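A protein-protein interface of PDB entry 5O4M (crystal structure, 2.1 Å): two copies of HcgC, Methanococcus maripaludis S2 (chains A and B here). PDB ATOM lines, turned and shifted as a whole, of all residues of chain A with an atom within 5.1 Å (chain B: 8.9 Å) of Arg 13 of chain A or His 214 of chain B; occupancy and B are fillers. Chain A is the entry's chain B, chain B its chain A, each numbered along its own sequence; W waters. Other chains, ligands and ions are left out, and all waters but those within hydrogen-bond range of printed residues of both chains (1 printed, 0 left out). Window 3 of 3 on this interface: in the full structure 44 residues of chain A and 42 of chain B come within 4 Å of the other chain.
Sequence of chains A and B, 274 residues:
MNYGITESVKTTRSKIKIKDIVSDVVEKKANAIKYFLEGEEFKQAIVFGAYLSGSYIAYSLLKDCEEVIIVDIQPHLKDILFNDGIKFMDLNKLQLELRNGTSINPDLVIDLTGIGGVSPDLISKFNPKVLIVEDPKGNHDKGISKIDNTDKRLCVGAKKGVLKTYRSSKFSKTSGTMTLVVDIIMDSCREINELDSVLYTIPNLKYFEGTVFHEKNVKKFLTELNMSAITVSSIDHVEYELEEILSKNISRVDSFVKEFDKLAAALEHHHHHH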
ATOM      1  N   ASN A   2       5.885  27.696 -15.753  1.00  0.00           N
ATOM      2  CA  ASN A   2       6.908  27.086 -14.887  1.00  0.00           C
ATOM      3  C   ASN A   2       7.024  25.569 -15.078  1.00  0.00           C
ATOM      4  O   ASN A   2       6.281  24.984 -15.852  1.00  0.00           O
ATOM      5  CB  ASN A   2       6.695  27.474 -13.417  1.00  0.00           C
ATOM      6  CG  ASN A   2       5.343  27.190 -12.852  1.00  0.00           C
ATOM      7  OD1 ASN A   2       4.555  28.109 -12.652  1.00  0.00           O
ATOM      8  ND2 ASN A   2       5.104  25.949 -12.426  1.00  0.00           N
ATOM      9  N   TYR A   3       7.948  24.917 -14.384  1.00  0.00           N
ATOM     10  CA  TYR A   3       8.059  23.480 -14.537  1.00  0.00           C
ATOM     11  C   TYR A   3       6.983  22.845 -13.637  1.00  0.00           C
ATOM     12  O   TYR A   3       6.473  23.523 -12.728  1.00  0.00           O
ATOM     13  CB  TYR A   3       9.451  22.995 -14.143  1.00  0.00           C
ATOM     14  CG  TYR A   3      10.522  23.464 -15.091  1.00  0.00           C
ATOM     15  CD1 TYR A   3      10.490  23.112 -16.440  1.00  0.00           C
ATOM     16  CD2 TYR A   3      11.562  24.277 -14.654  1.00  0.00           C
ATOM     17  CE1 TYR A   3      11.491  23.524 -17.314  1.00  0.00           C
ATOM     18  CE2 TYR A   3      12.554  24.714 -15.524  1.00  0.00           C
ATOM     19  CZ  TYR A   3      12.515  24.337 -16.857  1.00  0.00           C
ATOM     20  OH  TYR A   3      13.483  24.759 -17.743  1.00  0.00           O
ATOM     21  N   GLY A   4       6.652  21.573 -13.901  1.00  0.00           N
ATOM     22  CA  GLY A   4       5.658  20.828 -13.130  1.00  0.00           C
ATOM     23  C   GLY A   4       6.320  19.998 -12.048  1.00  0.00           C
ATOM     24  O   GLY A   4       7.025  20.535 -11.195  1.00  0.00           O
ATOM     25  N   THR A  11       4.016  23.849 -16.678  1.00  0.00           N
ATOM     26  CA  THR A  11       2.734  24.292 -16.110  1.00  0.00           C
ATOM     27  C   THR A  11       2.550  25.678 -16.634  1.00  0.00           C
ATOM     28  O   THR A  11       3.394  26.534 -16.431  1.00  0.00           O
ATOM     29  CB  THR A  11       2.720  24.305 -14.598  1.00  0.00           C
ATOM     30  OG1 THR A  11       2.828  22.965 -14.149  1.00  0.00           O
ATOM     31  CG2 THR A  11       1.417  24.891 -14.016  1.00  0.00           C
ATOM     32  N   THR A  12       1.434  25.912 -17.287  1.00  0.00           N
ATOM     33  CA  THR A  12       1.108  27.200 -17.847  1.00  0.00           C
ATOM     34  C   THR A  12      -0.195  27.672 -17.291  1.00  0.00           C
ATOM     35  O   THR A  12      -1.211  27.010 -17.449  1.00  0.00           O
ATOM     36  CB  THR A  12       1.061  27.088 -19.378  1.00  0.00           C
ATOM     37  OG1 THR A  12       2.292  26.544 -19.849  1.00  0.00           O
ATOM     38  CG2 THR A  12       0.812  28.443 -20.065  1.00  0.00           C
ATOM     39  N   ARG A  13      -0.184  28.829 -16.661  1.00  0.00           N
ATOM     40  CA  ARG A  13      -1.389  29.422 -16.096  1.00  0.00           C
ATOM     41  C   ARG A  13      -1.798  30.472 -17.110  1.00  0.00           C
ATOM     42  O   ARG A  13      -0.952  31.259 -17.542  1.00  0.00           O
ATOM     43  CB  ARG A  13      -1.097  30.052 -14.744  1.00  0.00           C
ATOM     44  CG  ARG A  13      -0.886  29.034 -13.646  1.00  0.00           C
ATOM     45  CD  ARG A  13      -0.305  29.671 -12.417  1.00  0.00           C
ATOM     46  NE  ARG A  13      -0.034  28.687 -11.365  1.00  0.00           N
ATOM     47  CZ  ARG A  13       1.013  27.868 -11.316  1.00  0.00           C
ATOM     48  NH1 ARG A  13       1.151  27.021 -10.307  1.00  0.00           N
ATOM     49  NH2 ARG A  13       1.932  27.886 -12.278  1.00  0.00           N
ATOM     50  N   SER A  14      -3.067  30.492 -17.500  1.00  0.00           N
ATOM     51  CA  SER A  14      -3.528  31.473 -18.470  1.00  0.00           C
ATOM     52  C   SER A  14      -3.407  32.912 -17.991  1.00  0.00           C
ATOM     53  O   SER A  14      -3.644  33.205 -16.822  1.00  0.00           O
ATOM     54  CB  SER A  14      -4.972  31.204 -18.873  1.00  0.00           C
ATOM     55  OG  SER A  14      -5.859  31.480 -17.806  1.00  0.00           O
ATOM     56  N   LYS A  15      -3.073  33.807 -18.895  1.00  0.00           N
ATOM     57  CA  LYS A  15      -2.950  35.239 -18.601  1.00  0.00           C
ATOM     58  C   LYS A  15      -4.343  35.767 -18.359  1.00  0.00           C
ATOM     59  O   LYS A  15      -4.552  36.584 -17.457  1.00  0.00           O
ATOM     60  CB  LYS A  15      -2.242  35.978 -19.727  1.00  0.00           C
ATOM     61  CG  LYS A  15      -0.816  35.529 -19.905  1.00  0.00           C
ATOM     62  CD  LYS A  15       0.108  36.036 -18.799  1.00  0.00           C
ATOM     63  CE  LYS A  15       1.373  35.209 -18.693  1.00  0.00           C
ATOM     64  NZ  LYS A  15       2.246  35.355 -19.890  1.00  0.00           N
ATOM     65  N   MET A 227      -7.897  34.653 -10.121  1.00  0.00           N
ATOM     66  CA  MET A 227      -7.213  33.443 -10.512  1.00  0.00           C
ATOM     67  C   MET A 227      -7.246  33.306 -12.039  1.00  0.00           C
ATOM     68  O   MET A 227      -8.193  33.773 -12.692  1.00  0.00           O
ATOM     69  CB  MET A 227      -7.934  32.240  -9.843  1.00  0.00           C
ATOM     70  CG  MET A 227      -7.219  30.902  -9.956  1.00  0.00           C
ATOM     71  SD  MET A 227      -5.719  30.812  -8.954  1.00  0.00           S
ATOM     72  CE  MET A 227      -4.480  30.293 -10.231  1.00  0.00           C
ATOM     73  N   SER A 228      -6.201  32.658 -12.594  1.00  0.00           N
ATOM     74  CA  SER A 228      -6.082  32.382 -14.021  1.00  0.00           C
ATOM     75  C   SER A 228      -7.270  31.498 -14.313  1.00  0.00           C
ATOM     76  O   SER A 228      -7.606  30.654 -13.466  1.00  0.00           O
ATOM     77  CB  SER A 228      -4.813  31.582 -14.319  1.00  0.00           C
ATOM     78  OG  SER A 228      -3.714  32.448 -14.258  1.00  0.00           O
ATOM     79  N   ILE A 230      -7.500  29.110 -16.612  1.00  0.00           N
ATOM     80  CA  ILE A 230      -7.040  27.753 -16.874  1.00  0.00           C
ATOM     81  C   ILE A 230      -5.581  27.548 -16.567  1.00  0.00           C
ATOM     82  O   ILE A 230      -4.774  28.445 -16.749  1.00  0.00           O
ATOM     83  CB  ILE A 230      -7.339  27.404 -18.389  1.00  0.00           C
ATOM     84  CG1 ILE A 230      -8.855  27.364 -18.655  1.00  0.00           C
ATOM     85  CG2 ILE A 230      -6.680  26.054 -18.838  1.00  0.00           C
ATOM     86  CD1 ILE A 230      -9.255  27.336 -20.079  1.00  0.00           C
ATOM     87  N   THR A 231      -5.253  26.340 -16.115  1.00  0.00           N
ATOM     88  CA  THR A 231      -3.910  25.902 -15.804  1.00  0.00           C
ATOM     89  C   THR A 231      -3.720  24.624 -16.613  1.00  0.00           C
ATOM     90  O   THR A 231      -4.552  23.732 -16.552  1.00  0.00           O
ATOM     91  CB  THR A 231      -3.670  25.734 -14.309  1.00  0.00           C
ATOM     92  OG1 THR A 231      -3.950  26.992 -13.695  1.00  0.00           O
ATOM     93  CG2 THR A 231      -2.217  25.312 -14.002  1.00  0.00           C
ATOM     94  N   VAL A 232      -2.643  24.545 -17.378  1.00  0.00           N
ATOM     95  CA  VAL A 232      -2.348  23.392 -18.217  1.00  0.00           C
ATOM     96  C   VAL A 232      -1.004  22.770 -17.903  1.00  0.00           C
ATOM     97  O   VAL A 232      -0.050  23.488 -17.666  1.00  0.00           O
ATOM     98  CB  VAL A 232      -2.288  23.818 -19.705  1.00  0.00           C
ATOM     99  CG1 VAL A 232      -2.318  22.596 -20.614  1.00  0.00           C
ATOM    100  CG2 VAL A 232      -3.408  24.789 -20.061  1.00  0.00           C
ATOM    101  N   LEU A 242      -3.380  28.639 -25.758  1.00  0.00           N
ATOM    102  CA  LEU A 242      -4.250  28.701 -24.592  1.00  0.00           C
ATOM    103  C   LEU A 242      -5.038  30.045 -24.604  1.00  0.00           C
ATOM    104  O   LEU A 242      -6.259  30.041 -24.425  1.00  0.00           O
ATOM    105  CB  LEU A 242      -3.404  28.505 -23.333  1.00  0.00           C
ATOM    106  CG  LEU A 242      -3.941  28.948 -21.967  1.00  0.00           C
ATOM    107  CD1 LEU A 242      -5.196  28.231 -21.612  1.00  0.00           C
ATOM    108  CD2 LEU A 242      -2.908  28.650 -20.896  1.00  0.00           C
ATOM    109  N   GLU A 243      -4.347  31.177 -24.840  1.00  0.00           N
ATOM    110  CA  GLU A 243      -5.003  32.493 -24.881  1.00  0.00           C
ATOM    111  C   GLU A 243      -5.929  32.632 -26.104  1.00  0.00           C
ATOM    112  O   GLU A 243      -6.991  33.237 -25.996  1.00  0.00           O
ATOM    113  CB  GLU A 243      -3.979  33.647 -24.883  1.00  0.00           C
ATOM    114  CG  GLU A 243      -3.031  33.706 -23.700  1.00  0.00           C
ATOM    115  CD  GLU A 243      -3.564  33.335 -22.325  1.00  0.00           C
ATOM    116  OE1 GLU A 243      -4.627  33.861 -21.919  1.00  0.00           O
ATOM    117  OE2 GLU A 243      -2.851  32.597 -21.607  1.00  0.00           O
ATOM    118  N   GLN B  74      11.768  14.029  -4.045  1.00  0.00           N
ATOM    119  CA  GLN B  74      11.271  15.094  -3.167  1.00  0.00           C
ATOM    120  C   GLN B  74      11.230  14.600  -1.716  1.00  0.00           C
ATOM    121  O   GLN B  74      10.328  13.828  -1.386  1.00  0.00           O
ATOM    122  CB  GLN B  74       9.848  15.513  -3.586  1.00  0.00           C
ATOM    123  CG  GLN B  74       9.708  16.035  -5.007  1.00  0.00           C
ATOM    124  CD  GLN B  74      10.341  17.382  -5.233  1.00  0.00           C
ATOM    125  OE1 GLN B  74      10.438  18.223  -4.335  1.00  0.00           O
ATOM    126  NE2 GLN B  74      10.740  17.639  -6.458  1.00  0.00           N
ATOM    127  N   HIS B  76      10.112  15.977   1.013  1.00  0.00           N
ATOM    128  CA  HIS B  76       8.874  16.326   1.715  1.00  0.00           C
ATOM    129  C   HIS B  76       7.713  15.344   1.421  1.00  0.00           C
ATOM    130  O   HIS B  76       6.736  15.347   2.161  1.00  0.00           O
ATOM    131  CB  HIS B  76       8.452  17.775   1.435  1.00  0.00           C
ATOM    132  CG  HIS B  76       7.774  17.945   0.118  1.00  0.00           C
ATOM    133  ND1 HIS B  76       8.493  18.001  -1.055  1.00  0.00           N
ATOM    134  CD2 HIS B  76       6.462  18.047  -0.167  1.00  0.00           C
ATOM    135  CE1 HIS B  76       7.600  18.145  -2.019  1.00  0.00           C
ATOM    136  NE2 HIS B  76       6.362  18.176  -1.530  1.00  0.00           N
ATOM    137  N   LYS B 206      -8.621  22.535  -9.378  1.00  0.00           N
ATOM    138  CA  LYS B 206      -7.520  23.484  -9.232  1.00  0.00           C
ATOM    139  C   LYS B 206      -6.266  22.700  -9.564  1.00  0.00           C
ATOM    140  O   LYS B 206      -6.321  21.475  -9.777  1.00  0.00           O
ATOM    141  CB  LYS B 206      -7.464  24.071  -7.818  1.00  0.00           C
ATOM    142  CG  LYS B 206      -7.059  23.117  -6.727  1.00  0.00           C
ATOM    143  CD  LYS B 206      -6.726  23.880  -5.439  1.00  0.00           C
ATOM    144  CE  LYS B 206      -5.328  24.467  -5.464  1.00  0.00           C
ATOM    145  NZ  LYS B 206      -5.124  25.464  -4.386  1.00  0.00           N
ATOM    146  N   TYR B 207      -5.163  23.385  -9.621  1.00  0.00           N
ATOM    147  CA  TYR B 207      -3.877  22.782  -9.915  1.00  0.00           C
ATOM    148  C   TYR B 207      -3.338  22.225  -8.613  1.00  0.00           C
ATOM    149  O   TYR B 207      -2.458  22.816  -7.970  1.00  0.00           O
ATOM    150  CB  TYR B 207      -2.966  23.827 -10.561  1.00  0.00           C
ATOM    151  CG  TYR B 207      -1.571  23.323 -10.864  1.00  0.00           C
ATOM    152  CD1 TYR B 207      -1.367  22.171 -11.607  1.00  0.00           C
ATOM    153  CD2 TYR B 207      -0.453  24.042 -10.463  1.00  0.00           C
ATOM    154  CE1 TYR B 207      -0.085  21.727 -11.908  1.00  0.00           C
ATOM    155  CE2 TYR B 207       0.827  23.586 -10.720  1.00  0.00           C
ATOM    156  CZ  TYR B 207       1.015  22.427 -11.440  1.00  0.00           C
ATOM    157  OH  TYR B 207       2.314  22.028 -11.697  1.00  0.00           O
ATOM    158  N   PHE B 208      -3.888  21.083  -8.230  1.00  0.00           N
ATOM    159  CA  PHE B 208      -3.543  20.351  -6.982  1.00  0.00           C
ATOM    160  C   PHE B 208      -2.081  19.953  -6.921  1.00  0.00           C
ATOM    161  O   PHE B 208      -1.475  19.933  -5.843  1.00  0.00           O
ATOM    162  CB  PHE B 208      -4.376  19.075  -6.866  1.00  0.00           C
ATOM    163  CG  PHE B 208      -5.875  19.243  -6.883  1.00  0.00           C
ATOM    164  CD1 PHE B 208      -6.553  19.727  -5.766  1.00  0.00           C
ATOM    165  CD2 PHE B 208      -6.616  18.863  -7.986  1.00  0.00           C
ATOM    166  CE1 PHE B 208      -7.935  19.852  -5.776  1.00  0.00           C
ATOM    167  CE2 PHE B 208      -8.001  19.004  -7.994  1.00  0.00           C
ATOM    168  CZ  PHE B 208      -8.649  19.498  -6.890  1.00  0.00           C
ATOM    169  N   GLU B 209      -1.524  19.625  -8.082  1.00  0.00           N
ATOM    170  CA  GLU B 209      -0.136  19.211  -8.245  1.00  0.00           C
ATOM    171  C   GLU B 209       0.792  20.331  -7.786  1.00  0.00           C
ATOM    172  O   GLU B 209       1.854  20.033  -7.312  1.00  0.00           O
ATOM    173  CB  GLU B 209       0.120  18.830  -9.712  1.00  0.00           C
ATOM    174  CG  GLU B 209       1.573  18.805 -10.165  1.00  0.00           C
ATOM    175  CD  GLU B 209       1.609  18.617 -11.667  1.00  0.00           C
ATOM    176  OE1 GLU B 209       0.984  17.653 -12.167  1.00  0.00           O
ATOM    177  OE2 GLU B 209       2.293  19.416 -12.338  1.00  0.00           O
ATOM    178  N   GLY B 210       0.397  21.595  -7.964  1.00  0.00           N
ATOM    179  CA  GLY B 210       1.168  22.762  -7.517  1.00  0.00           C
ATOM    180  C   GLY B 210       1.253  22.819  -6.004  1.00  0.00           C
ATOM    181  O   GLY B 210       2.285  23.175  -5.448  1.00  0.00           O
ATOM    182  N   THR B 211       0.178  22.463  -5.309  1.00  0.00           N
ATOM    183  CA  THR B 211       0.175  22.456  -3.842  1.00  0.00           C
ATOM    184  C   THR B 211       1.235  21.463  -3.312  1.00  0.00           C
ATOM    185  O   THR B 211       1.939  21.734  -2.350  1.00  0.00           O
ATOM    186  CB  THR B 211      -1.181  21.969  -3.316  1.00  0.00           C
ATOM    187  OG1 THR B 211      -2.213  22.692  -3.926  1.00  0.00           O
ATOM    188  CG2 THR B 211      -1.312  22.084  -1.813  1.00  0.00           C
ATOM    189  N   VAL B 212       1.326  20.306  -3.950  1.00  0.00           N
ATOM    190  CA  VAL B 212       2.258  19.253  -3.567  1.00  0.00           C
ATOM    191  C   VAL B 212       3.683  19.554  -3.935  1.00  0.00           C
ATOM    192  O   VAL B 212       4.538  19.340  -3.108  1.00  0.00           O
ATOM    193  CB  VAL B 212       1.844  17.875  -4.213  1.00  0.00           C
ATOM    194  CG1 VAL B 212       2.842  16.764  -3.893  1.00  0.00           C
ATOM    195  CG2 VAL B 212       0.478  17.461  -3.749  1.00  0.00           C
ATOM    196  N   PHE B 213       3.964  20.008  -5.185  1.00  0.00           N
ATOM    197  CA  PHE B 213       5.339  20.248  -5.658  1.00  0.00           C
ATOM    198  C   PHE B 213       5.892  21.690  -5.689  1.00  0.00           C
ATOM    199  O   PHE B 213       7.116  21.875  -5.797  1.00  0.00           O
ATOM    200  CB  PHE B 213       5.463  19.658  -7.072  1.00  0.00           C
ATOM    201  CG  PHE B 213       5.190  18.182  -7.032  1.00  0.00           C
ATOM    202  CD1 PHE B 213       6.214  17.277  -6.755  1.00  0.00           C
ATOM    203  CD2 PHE B 213       3.908  17.694  -7.209  1.00  0.00           C
ATOM    204  CE1 PHE B 213       5.955  15.922  -6.660  1.00  0.00           C
ATOM    205  CE2 PHE B 213       3.643  16.331  -7.117  1.00  0.00           C
ATOM    206  CZ  PHE B 213       4.672  15.450  -6.839  1.00  0.00           C
ATOM    207  N   HIS B 214       5.041  22.681  -5.649  1.00  0.00           N
ATOM    208  CA  HIS B 214       5.521  24.054  -5.672  1.00  0.00           C
ATOM    209  C   HIS B 214       5.422  24.595  -4.251  1.00  0.00           C
ATOM    210  O   HIS B 214       6.407  25.091  -3.717  1.00  0.00           O
ATOM    211  CB  HIS B 214       4.705  24.916  -6.654  1.00  0.00           C
ATOM    212  CG  HIS B 214       4.698  24.493  -8.085  1.00  0.00           C
ATOM    213  ND1 HIS B 214       5.262  23.301  -8.529  1.00  0.00           N
ATOM    214  CD2 HIS B 214       4.157  25.135  -9.150  1.00  0.00           C
ATOM    215  CE1 HIS B 214       5.024  23.254  -9.827  1.00  0.00           C
ATOM    216  NE2 HIS B 214       4.418  24.360 -10.253  1.00  0.00           N
ATOM    217  N   GLU B 215       4.226  24.496  -3.636  1.00  0.00           N
ATOM    218  CA  GLU B 215       4.015  24.956  -2.261  1.00  0.00           C
ATOM    219  C   GLU B 215       4.618  23.957  -1.297  1.00  0.00           C
ATOM    220  O   GLU B 215       4.935  24.333  -0.177  1.00  0.00           O
ATOM    221  CB  GLU B 215       2.525  25.166  -1.955  1.00  0.00           C
ATOM    222  CG  GLU B 215       1.926  26.265  -2.805  1.00  0.00           C
ATOM    223  CD  GLU B 215       0.421  26.355  -2.775  1.00  0.00           C
ATOM    224  OE1 GLU B 215      -0.138  27.028  -3.673  1.00  0.00           O
ATOM    225  OE2 GLU B 215      -0.200  25.719  -1.887  1.00  0.00           O
ATOM    226  N   LYS B 216       4.782  22.690  -1.728  1.00  0.00           N
ATOM    227  CA  LYS B 216       5.359  21.603  -0.919  1.00  0.00           C
ATOM    228  C   LYS B 216       4.552  21.380   0.365  1.00  0.00           C
ATOM    229  O   LYS B 216       5.118  21.234   1.445  1.00  0.00           O
ATOM    230  CB  LYS B 216       6.855  21.857  -0.681  1.00  0.00           C
ATOM    231  CG  LYS B 216       7.614  21.856  -2.010  1.00  0.00           C
ATOM    232  CD  LYS B 216       9.123  22.075  -1.822  1.00  0.00           C
ATOM    233  CE  LYS B 216       9.960  21.340  -2.827  1.00  0.00           C
ATOM    234  NZ  LYS B 216       9.641  21.711  -4.225  1.00  0.00           N
ATOM    235  N   ASN B 217       3.214  21.360   0.223  1.00  0.00           N
ATOM    236  CA  ASN B 217       2.293  21.171   1.343  1.00  0.00           C
ATOM    237  C   ASN B 217       1.309  20.018   1.115  1.00  0.00           C
ATOM    238  O   ASN B 217       0.203  20.233   0.618  1.00  0.00           O
ATOM    239  CB  ASN B 217       1.554  22.482   1.608  1.00  0.00           C
ATOM    240  CG  ASN B 217       0.898  22.532   2.976  1.00  0.00           C
ATOM    241  OD1 ASN B 217       0.520  21.517   3.553  1.00  0.00           O
ATOM    242  ND2 ASN B 217       0.637  23.720   3.463  1.00  0.00           N
ATOM    243  N   VAL B 218       1.705  18.805   1.500  1.00  0.00           N
ATOM    244  CA  VAL B 218       0.865  17.595   1.346  1.00  0.00           C
ATOM    245  C   VAL B 218      -0.428  17.736   2.152  1.00  0.00           C
ATOM    246  O   VAL B 218      -1.488  17.406   1.653  1.00  0.00           O
ATOM    247  CB  VAL B 218       1.641  16.320   1.759  1.00  0.00           C
ATOM    248  CG1 VAL B 218       0.717  15.115   1.866  1.00  0.00           C
ATOM    249  CG2 VAL B 218       2.778  16.041   0.782  1.00  0.00           C
HETATM  250  O   HOH W   1       2.504  20.315 -14.758  1.00  0.00           O
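No position is printed for both chains.
Of the 9 pairs that touch across the chains among the printed residues, none has its exchanged pair printed and touching as well.
Water W1 bridges the side-chain carboxylate of Glu 209 of chain B (2.6 Å) and the side-chain hydroxyl of Thr 11 of chain A (2.7 Å).
The side-chain carboxylate (OE2) of Glu 209 of chain B lies within hydrogen-bond range of the side-chain hydroxyl (OH) of Tyr 207 of chain B, 2.7 Å away.
The guanidinium group (NH2) of Arg 13 of chain A is in hydrogen-bond range of the side-chain amide oxygen (OD1) of Asn 2 of chain A (2.7 Å).
OH of Tyr 207 of chain B lies within hydrogen-bond range of NE2 of His 214 of chain B (3.5 Å).
O of Asn 2 of chain A lies within hydrogen-bond range of N of Thr 11 of chain A.
The side-chain amide nitrogen (ND2) of Asn 2 of chain A sits at hydrogen-bond distance from a ring nitrogen (NE2) of His 214 of chain B (2.8 Å).
OH of Tyr 207 of chain B sits at hydrogen-bond distance from OG1 of Thr 11 of chain A, at 2.7 Å.
NE2 of His 214 of chain B sits close to O of Tyr 3 of chain A, at 3.3 Å.
CA of Gly 4 of chain A touches OH of Tyr 207 of chain B (3.8 Å).
Gly 4 of chain A touches Glu 209 of chain B (CA to OE2, 3.7 Å).
Gly 4 of chain A touches His 214 of chain B (O to CE1, 3.6 Å).
CD2 of Tyr 207 of chain B touches NH1 of Arg 13 of chain A, at 3.4 Å.
Arg 13 of chain A touches His 214 of chain B (NH1 to CD2, 3.7 Å).
CG2 of Thr 231 of chain A touches CG of Tyr 207 of chain B, 3.8 Å away.
Of the printed residues of chain B, Tyr 3 of chain A touches His 214.
Of chain B, only Tyr 207 (3.8 Å), Glu 209 (3.7 Å) and His 214 (3.6 Å) come within 4 Å of Gly 4 of chain A.
Arg 13 of chain A touches two residues of chain B.
No residue of chain B comes within 4 Å of Ser 14 of chain A.
Glu 243 of chain A touches none of the printed residues of chain B.
His 76 of chain B touches none of the printed residues of chain A.
Printed residues of chain A within 4 Å of Glu 209 of chain B: Gly 4.
The nearest residue of chain B that does not touch Arg 13 of chain A is Gly 210 of chain B (5.1 Å).
The nearest residue of chain A that does not touch His 214 of chain B is Thr 11 of chain A (4.4 Å).
The nearest printed residue of chain B that does not touch Asn 2 of chain A is Tyr 207 of chain B (4.9 Å).
Along chain A the printed residues that touch a printed residue of chain B span positions 2 to 231.
Printed residues of chain B that touch a printed residue of chain A: Tyr 207, Glu 209 and His 214.
Among the printed residues, no Asp or Glu carboxylate lies within 4 Å of a Lys or Arg side-chain nitrogen of the other chain.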
